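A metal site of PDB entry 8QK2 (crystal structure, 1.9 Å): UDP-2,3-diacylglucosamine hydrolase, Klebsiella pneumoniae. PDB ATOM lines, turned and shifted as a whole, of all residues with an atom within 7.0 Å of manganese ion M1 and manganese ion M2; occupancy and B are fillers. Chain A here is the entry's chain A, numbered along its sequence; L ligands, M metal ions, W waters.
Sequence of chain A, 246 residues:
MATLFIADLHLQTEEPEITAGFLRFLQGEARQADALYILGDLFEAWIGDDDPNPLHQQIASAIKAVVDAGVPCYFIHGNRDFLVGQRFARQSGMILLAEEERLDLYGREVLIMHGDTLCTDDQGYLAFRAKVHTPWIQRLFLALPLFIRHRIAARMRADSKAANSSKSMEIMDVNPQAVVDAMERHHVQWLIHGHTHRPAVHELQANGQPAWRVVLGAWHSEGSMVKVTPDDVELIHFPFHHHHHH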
ATOM      1  N   ALA A   7      28.624   4.173  -5.218  1.00  0.00           N
ATOM      2  CA  ALA A   7      28.974   2.804  -5.565  1.00  0.00           C
ATOM      3  C   ALA A   7      28.762   2.572  -7.064  1.00  0.00           C
ATOM      4  O   ALA A   7      28.174   3.422  -7.743  1.00  0.00           O
ATOM      5  CB  ALA A   7      28.170   1.839  -4.721  1.00  0.00           C
ATOM      6  N   ASP A   8      29.260   1.426  -7.557  1.00  0.00           N
ATOM      7  CA  ASP A   8      28.913   0.941  -8.878  1.00  0.00           C
ATOM      8  C   ASP A   8      29.318   1.936  -9.979  1.00  0.00           C
ATOM      9  O   ASP A   8      28.597   2.088 -10.969  1.00  0.00           O
ATOM     10  CB  ASP A   8      27.427   0.563  -8.964  1.00  0.00           C
ATOM     11  CG  ASP A   8      27.048  -0.516  -7.976  1.00  0.00           C
ATOM     12  OD1 ASP A   8      27.519  -1.646  -8.135  1.00  0.00           O
ATOM     13  OD2 ASP A   8      26.314  -0.221  -7.015  1.00  0.00           O
ATOM     14  N   LEU A   9      30.521   2.501  -9.841  1.00  0.00           N
ATOM     15  CA  LEU A   9      31.115   3.328 -10.887  1.00  0.00           C
ATOM     16  C   LEU A   9      31.610   2.488 -12.063  1.00  0.00           C
ATOM     17  O   LEU A   9      31.611   2.951 -13.201  1.00  0.00           O
ATOM     18  CB  LEU A   9      32.252   4.149 -10.283  1.00  0.00           C
ATOM     19  CG  LEU A   9      31.776   5.235  -9.301  1.00  0.00           C
ATOM     20  CD1 LEU A   9      31.718   4.724  -7.868  1.00  0.00           C
ATOM     21  CD2 LEU A   9      32.669   6.444  -9.390  1.00  0.00           C
ATOM     22  N   HIS A  10      32.028   1.245 -11.796  1.00  0.00           N
ATOM     23  CA  HIS A  10      32.492   0.332 -12.837  1.00  0.00           C
ATOM     24  C   HIS A  10      33.535   0.995 -13.743  1.00  0.00           C
ATOM     25  O   HIS A  10      33.458   0.886 -14.959  1.00  0.00           O
ATOM     26  CB  HIS A  10      31.292  -0.252 -13.594  1.00  0.00           C
ATOM     27  CG  HIS A  10      30.468  -1.155 -12.741  1.00  0.00           C
ATOM     28  ND1 HIS A  10      30.636  -2.526 -12.804  1.00  0.00           N
ATOM     29  CD2 HIS A  10      29.538  -0.939 -11.818  1.00  0.00           C
ATOM     30  CE1 HIS A  10      29.821  -3.103 -11.932  1.00  0.00           C
ATOM     31  NE2 HIS A  10      29.146  -2.156 -11.328  1.00  0.00           N
ATOM     32  N   LEU A  39      30.984   2.076  -1.804  1.00  0.00           N
ATOM     33  CA  LEU A  39      30.404   0.818  -1.406  1.00  0.00           C
ATOM     34  C   LEU A  39      30.523  -0.209  -2.528  1.00  0.00           C
ATOM     35  O   LEU A  39      29.573  -0.932  -2.833  1.00  0.00           O
ATOM     36  CB  LEU A  39      28.950   1.092  -1.006  1.00  0.00           C
ATOM     37  CG  LEU A  39      28.751   2.117   0.112  1.00  0.00           C
ATOM     38  CD1 LEU A  39      27.319   2.048   0.644  1.00  0.00           C
ATOM     39  CD2 LEU A  39      29.747   1.908   1.251  1.00  0.00           C
ATOM     40  N   GLY A  40      31.710  -0.270  -3.143  1.00  0.00           N
ATOM     41  CA  GLY A  40      32.076  -1.387  -3.992  1.00  0.00           C
ATOM     42  C   GLY A  40      31.785  -1.131  -5.465  1.00  0.00           C
ATOM     43  O   GLY A  40      31.033  -0.209  -5.789  1.00  0.00           O
ATOM     44  N   ASP A  41      32.396  -1.961  -6.321  1.00  0.00           N
ATOM     45  CA  ASP A  41      32.344  -1.836  -7.772  1.00  0.00           C
ATOM     46  C   ASP A  41      32.775  -0.428  -8.177  1.00  0.00           C
ATOM     47  O   ASP A  41      32.176   0.191  -9.051  1.00  0.00           O
ATOM     48  CB  ASP A  41      30.938  -2.186  -8.300  1.00  0.00           C
ATOM     49  CG  ASP A  41      30.566  -3.664  -8.223  1.00  0.00           C
ATOM     50  OD1 ASP A  41      31.432  -4.473  -7.788  1.00  0.00           O
ATOM     51  OD2 ASP A  41      29.381  -3.972  -8.588  1.00  0.00           O
ATOM     52  N   GLU A  44      35.481  -1.873 -12.747  1.00  0.00           N
ATOM     53  CA  GLU A  44      34.797  -2.901 -13.510  1.00  0.00           C
ATOM     54  C   GLU A  44      35.456  -4.263 -13.312  1.00  0.00           C
ATOM     55  O   GLU A  44      34.792  -5.294 -13.477  1.00  0.00           O
ATOM     56  CB  GLU A  44      34.809  -2.543 -15.003  1.00  0.00           C
ATOM     57  CG  GLU A  44      34.229  -3.606 -15.926  1.00  0.00           C
ATOM     58  CD  GLU A  44      32.800  -4.034 -15.654  1.00  0.00           C
ATOM     59  OE1 GLU A  44      32.070  -3.321 -14.917  1.00  0.00           O
ATOM     60  OE2 GLU A  44      32.409  -5.103 -16.167  1.00  0.00           O
ATOM     61  N   GLY A  78      33.185  -4.606  -3.821  1.00  0.00           N
ATOM     62  CA  GLY A  78      32.100  -5.196  -4.595  1.00  0.00           C
ATOM     63  C   GLY A  78      32.449  -6.603  -5.088  1.00  0.00           C
ATOM     64  O   GLY A  78      33.472  -7.161  -4.723  1.00  0.00           O
ATOM     65  N   ASN A  79      31.568  -7.173  -5.910  1.00  0.00           N
ATOM     66  CA  ASN A  79      31.834  -8.446  -6.551  1.00  0.00           C
ATOM     67  C   ASN A  79      32.904  -8.290  -7.627  1.00  0.00           C
ATOM     68  O   ASN A  79      33.585  -9.262  -7.984  1.00  0.00           O
ATOM     69  CB  ASN A  79      30.585  -9.094  -7.163  1.00  0.00           C
ATOM     70  CG  ASN A  79      29.826  -8.145  -8.054  1.00  0.00           C
ATOM     71  OD1 ASN A  79      29.483  -7.063  -7.593  1.00  0.00           O
ATOM     72  ND2 ASN A  79      29.575  -8.501  -9.300  1.00  0.00           N
ATOM     73  N   ARG A  80      33.015  -7.082  -8.195  1.00  0.00           N
ATOM     74  CA  ARG A  80      33.894  -6.870  -9.331  1.00  0.00           C
ATOM     75  C   ARG A  80      35.323  -6.635  -8.840  1.00  0.00           C
ATOM     76  O   ARG A  80      36.253  -7.046  -9.529  1.00  0.00           O
ATOM     77  CB  ARG A  80      33.442  -5.678 -10.184  1.00  0.00           C
ATOM     78  CG  ARG A  80      32.072  -5.829 -10.839  1.00  0.00           C
ATOM     79  CD  ARG A  80      31.900  -7.046 -11.721  1.00  0.00           C
ATOM     80  NE  ARG A  80      32.800  -7.093 -12.869  1.00  0.00           N
ATOM     81  CZ  ARG A  80      32.821  -8.066 -13.776  1.00  0.00           C
ATOM     82  NH1 ARG A  80      31.938  -9.058 -13.733  1.00  0.00           N
ATOM     83  NH2 ARG A  80      33.708  -8.037 -14.747  1.00  0.00           N
ATOM     84  N   HIS A 114      28.019  -3.611   0.136  1.00  0.00           N
ATOM     85  CA  HIS A 114      27.877  -3.600  -1.318  1.00  0.00           C
ATOM     86  C   HIS A 114      26.450  -3.982  -1.729  1.00  0.00           C
ATOM     87  O   HIS A 114      25.861  -3.307  -2.574  1.00  0.00           O
ATOM     88  CB  HIS A 114      28.896  -4.486  -2.035  1.00  0.00           C
ATOM     89  CG  HIS A 114      28.833  -4.341  -3.515  1.00  0.00           C
ATOM     90  ND1 HIS A 114      28.995  -3.118  -4.147  1.00  0.00           N
ATOM     91  CD2 HIS A 114      28.543  -5.229  -4.488  1.00  0.00           C
ATOM     92  CE1 HIS A 114      28.849  -3.299  -5.450  1.00  0.00           C
ATOM     93  NE2 HIS A 114      28.585  -4.576  -5.681  1.00  0.00           N
ATOM     94  N   GLY A 115      25.944  -5.083  -1.157  1.00  0.00           N
ATOM     95  CA  GLY A 115      24.578  -5.533  -1.397  1.00  0.00           C
ATOM     96  C   GLY A 115      24.519  -6.902  -2.047  1.00  0.00           C
ATOM     97  O   GLY A 115      23.476  -7.568  -2.003  1.00  0.00           O
ATOM     98  N   ASP A 116      25.637  -7.371  -2.615  1.00  0.00           N
ATOM     99  CA  ASP A 116      25.674  -8.670  -3.269  1.00  0.00           C
ATOM    100  C   ASP A 116      25.356  -9.800  -2.287  1.00  0.00           C
ATOM    101  O   ASP A 116      24.743 -10.798  -2.691  1.00  0.00           O
ATOM    102  CB  ASP A 116      27.008  -8.890  -3.994  1.00  0.00           C
ATOM    103  CG  ASP A 116      28.213  -8.914  -3.069  1.00  0.00           C
ATOM    104  OD1 ASP A 116      28.458  -7.891  -2.373  1.00  0.00           O
ATOM    105  OD2 ASP A 116      28.899  -9.969  -3.023  1.00  0.00           O
ATOM    106  N   TYR A 125      26.006 -17.134  -8.214  1.00  0.00           N
ATOM    107  CA  TYR A 125      26.840 -16.050  -7.741  1.00  0.00           C
ATOM    108  C   TYR A 125      27.454 -16.414  -6.379  1.00  0.00           C
ATOM    109  O   TYR A 125      28.663 -16.242  -6.180  1.00  0.00           O
ATOM    110  CB  TYR A 125      26.101 -14.715  -7.623  1.00  0.00           C
ATOM    111  CG  TYR A 125      26.999 -13.707  -6.976  1.00  0.00           C
ATOM    112  CD1 TYR A 125      28.181 -13.343  -7.588  1.00  0.00           C
ATOM    113  CD2 TYR A 125      26.769 -13.246  -5.687  1.00  0.00           C
ATOM    114  CE1 TYR A 125      29.087 -12.495  -6.969  1.00  0.00           C
ATOM    115  CE2 TYR A 125      27.656 -12.389  -5.058  1.00  0.00           C
ATOM    116  CZ  TYR A 125      28.827 -12.028  -5.701  1.00  0.00           C
ATOM    117  OH  TYR A 125      29.739 -11.202  -5.088  1.00  0.00           O
ATOM    118  N   ILE A 171      21.606  -8.333 -13.193  1.00  0.00           N
ATOM    119  CA  ILE A 171      22.066  -8.604 -11.845  1.00  0.00           C
ATOM    120  C   ILE A 171      20.835  -8.934 -10.990  1.00  0.00           C
ATOM    121  O   ILE A 171      19.896  -8.161 -10.943  1.00  0.00           O
ATOM    122  CB  ILE A 171      22.881  -7.397 -11.314  1.00  0.00           C
ATOM    123  CG1 ILE A 171      24.148  -7.184 -12.159  1.00  0.00           C
ATOM    124  CG2 ILE A 171      23.208  -7.555  -9.840  1.00  0.00           C
ATOM    125  CD1 ILE A 171      24.955  -5.970 -11.764  1.00  0.00           C
ATOM    126  N   GLY A 194      24.513  -0.776  -2.866  1.00  0.00           N
ATOM    127  CA  GLY A 194      24.447  -0.722  -4.321  1.00  0.00           C
ATOM    128  C   GLY A 194      24.242  -2.119  -4.896  1.00  0.00           C
ATOM    129  O   GLY A 194      23.333  -2.842  -4.481  1.00  0.00           O
ATOM    130  N   HIS A 195      25.110  -2.484  -5.853  1.00  0.00           N
ATOM    131  CA  HIS A 195      25.164  -3.793  -6.487  1.00  0.00           C
ATOM    132  C   HIS A 195      24.030  -4.030  -7.504  1.00  0.00           C
ATOM    133  O   HIS A 195      24.299  -4.515  -8.602  1.00  0.00           O
ATOM    134  CB  HIS A 195      25.221  -4.945  -5.469  1.00  0.00           C
ATOM    135  CG  HIS A 195      25.332  -6.257  -6.160  1.00  0.00           C
ATOM    136  ND1 HIS A 195      26.373  -6.587  -6.996  1.00  0.00           N
ATOM    137  CD2 HIS A 195      24.480  -7.287  -6.191  1.00  0.00           C
ATOM    138  CE1 HIS A 195      26.159  -7.804  -7.483  1.00  0.00           C
ATOM    139  NE2 HIS A 195      25.027  -8.253  -7.003  1.00  0.00           N
ATOM    140  N   THR A 196      22.782  -3.774  -7.104  1.00  0.00           N
ATOM    141  CA  THR A 196      21.620  -4.188  -7.873  1.00  0.00           C
ATOM    142  C   THR A 196      21.353  -3.235  -9.045  1.00  0.00           C
ATOM    143  O   THR A 196      20.549  -3.567  -9.909  1.00  0.00           O
ATOM    144  CB  THR A 196      20.361  -4.313  -7.000  1.00  0.00           C
ATOM    145  OG1 THR A 196      19.998  -3.043  -6.448  1.00  0.00           O
ATOM    146  CG2 THR A 196      20.508  -5.302  -5.866  1.00  0.00           C
ATOM    147  N   HIS A 197      21.995  -2.053  -9.032  1.00  0.00           N
ATOM    148  CA  HIS A 197      21.846  -1.049 -10.089  1.00  0.00           C
ATOM    149  C   HIS A 197      20.381  -0.618 -10.256  1.00  0.00           C
ATOM    150  O   HIS A 197      19.997  -0.240 -11.348  1.00  0.00           O
ATOM    151  CB  HIS A 197      22.437  -1.543 -11.424  1.00  0.00           C
ATOM    152  CG  HIS A 197      23.903  -1.878 -11.396  1.00  0.00           C
ATOM    153  ND1 HIS A 197      24.609  -2.286 -12.507  1.00  0.00           N
ATOM    154  CD2 HIS A 197      24.790  -1.823 -10.387  1.00  0.00           C
ATOM    155  CE1 HIS A 197      25.864  -2.511 -12.164  1.00  0.00           C
ATOM    156  NE2 HIS A 197      26.005  -2.240 -10.880  1.00  0.00           N
ATOM    157  N   ALA A 218      24.188   2.696 -10.629  1.00  0.00           N
ATOM    158  CA  ALA A 218      25.424   2.605 -11.377  1.00  0.00           C
ATOM    159  C   ALA A 218      25.676   3.900 -12.134  1.00  0.00           C
ATOM    160  O   ALA A 218      24.754   4.650 -12.465  1.00  0.00           O
ATOM    161  CB  ALA A 218      25.365   1.415 -12.308  1.00  0.00           C
HETATM  162  C1  LIG L   1      40.304 -15.365  -8.181  1.00  0.00           C
HETATM  163  C2  LIG L   1      40.480 -16.559  -8.836  1.00  0.00           C
HETATM  164  N1  LIG L   1      39.298 -13.216 -10.899  1.00  0.00           N
HETATM  165  C3  LIG L   1      39.664 -11.967 -10.286  1.00  0.00           C
HETATM  166  C4  LIG L   1      38.602 -10.959 -10.706  1.00  0.00           C
HETATM  167  C5  LIG L   1      39.518 -13.187 -12.317  1.00  0.00           C
HETATM  168  C6  LIG L   1      38.479 -12.193 -12.899  1.00  0.00           C
HETATM  169  C7  LIG L   1      40.238 -16.627 -10.209  1.00  0.00           C
HETATM  170  N2  LIG L   1      39.883 -15.521 -10.881  1.00  0.00           N
HETATM  171  C8  LIG L   1      39.807 -14.337 -10.244  1.00  0.00           C
HETATM  172  N3  LIG L   1      39.950 -14.275  -8.900  1.00  0.00           N
HETATM  173  N4  LIG L   1      38.586 -10.846 -12.192  1.00  0.00           N
HETATM  174  S1  LIG L   1      37.389  -9.791 -12.683  1.00  0.00           S
HETATM  175  C9  LIG L   1      35.790 -10.485 -12.406  1.00  0.00           C
HETATM  176  O1  LIG L   1      37.550  -8.553 -11.958  1.00  0.00           O
HETATM  177  O2  LIG L   1      37.571  -9.575 -14.063  1.00  0.00           O
HETATM  178  C10 LIG L   1      35.277 -11.334 -13.336  1.00  0.00           C
HETATM  179  C11 LIG L   1      34.043 -11.919 -13.145  1.00  0.00           C
HETATM  180  C12 LIG L   1      33.271 -11.635 -12.023  1.00  0.00           C
HETATM  181  C13 LIG L   1      35.034 -10.168 -11.232  1.00  0.00           C
HETATM  182  C14 LIG L   1      33.767 -10.765 -11.050  1.00  0.00           C
HETATM  183  N5  LIG L   1      32.060 -12.330 -11.886  1.00  0.00           N
HETATM  184  C15 LIG L   1      31.036 -11.988 -11.029  1.00  0.00           C
HETATM  185  O3  LIG L   1      31.105 -10.999 -10.313  1.00  0.00           O
HETATM  186  C16 LIG L   1      29.798 -12.877 -11.026  1.00  0.00           C
HETATM  187  C17 LIG L   1      29.956 -14.256 -11.006  1.00  0.00           C
HETATM  188  C18 LIG L   1      28.832 -15.079 -11.035  1.00  0.00           C
HETATM  189  C19 LIG L   1      27.565 -14.534 -11.129  1.00  0.00           C
HETATM  190  C20 LIG L   1      27.401 -13.154 -11.173  1.00  0.00           C
HETATM  191  C21 LIG L   1      28.519 -12.313 -11.151  1.00  0.00           C
HETATM  192  N6  LIG L   1      28.345 -10.863 -11.141  1.00  0.00           N
HETATM  193  C22 LIG L   1      27.045 -10.481 -10.547  1.00  0.00           C
HETATM  194  S2  LIG L   1      28.485 -10.243 -12.645  1.00  0.00           S
HETATM  195  C23 LIG L   1      27.033 -10.638 -13.600  1.00  0.00           C
HETATM  196  O4  LIG L   1      28.648  -8.822 -12.552  1.00  0.00           O
HETATM  197  O5  LIG L   1      29.624 -10.790 -13.269  1.00  0.00           O
HETATM  198  C24 LIG L   1      40.520 -15.240  -6.680  1.00  0.00           C
HETATM  199  C25 LIG L   1      40.409 -17.846 -10.903  1.00  0.00           C
HETATM  200  N7  LIG L   1      40.512 -18.751 -11.579  1.00  0.00           N
HETATM  201 MN    MN M   1      28.125  -5.433  -7.694  1.00  0.00          MN
HETATM  202 MN    MN M   2      27.802  -2.898  -9.777  1.00  0.00          MN
HETATM  203  O   HOH W   1      26.837  -4.729  -9.297  1.00  0.00           O
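An oxygen (O3) of the ligand lies within hydrogen-bond range of the side-chain amide nitrogen of Asn 79 (3.1 Å).
O5 of the ligand sits at hydrogen-bond distance from NH1 of Arg 80 (2.9 Å).
OD2 of Asp 8 sits at hydrogen-bond distance from N of His 195.
The backbone carbonyl oxygen (O) of Gly 40 lies within hydrogen-bond range of the backbone NH (N) of Asp 8, at 3.0 Å.
The backbone NH (N) of Arg 80 lies within hydrogen-bond range of the side-chain carboxylate (OD1) of Asp 41, 3.1 Å away.
The backbone carbonyl oxygen (O) of Asp 41 is in hydrogen-bond range of the backbone NH (N) of Leu 9 (2.9 Å).
ND1 of His 10 lies within hydrogen-bond range of OE1 of Glu 44 (2.7 Å).
O of His 114 is in hydrogen-bond range of N of Gly 194 (2.9 Å).
ND1 of His 114 sits at hydrogen-bond distance from O of Leu 39 (2.6 Å).
Five residues have an atom within 4 Å of manganese ion M1: Asp 8, Asp 41, Asn 79, His 114 and His 195.
Four residues have an atom within 4 Å of manganese ion M2: Asp 8, His 10, Asp 41 and His 197.
The nearest printed residue that does not touch manganese ion M2 is His 195 (4.03 Å).
Manganese ion M1 is bound by the side-chain carboxylate of Asp 41 (2.1 Å), the side-chain amide oxygen of Asn 79 (2.1 Å), water W1 (2.2 Å), a ring nitrogen (ND1) of His 195 (2.2 Å) and a ring nitrogen (NE2) of His 114 (2.2 Å).
Manganese ion M2 is bound by OD1 of Asp 8 (2.1 Å), water W1 (2.1 Å), NE2 of His 10 (2.2 Å), NE2 of His 197 (2.2 Å) and OD2 of Asp 41 (2.2 Å).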
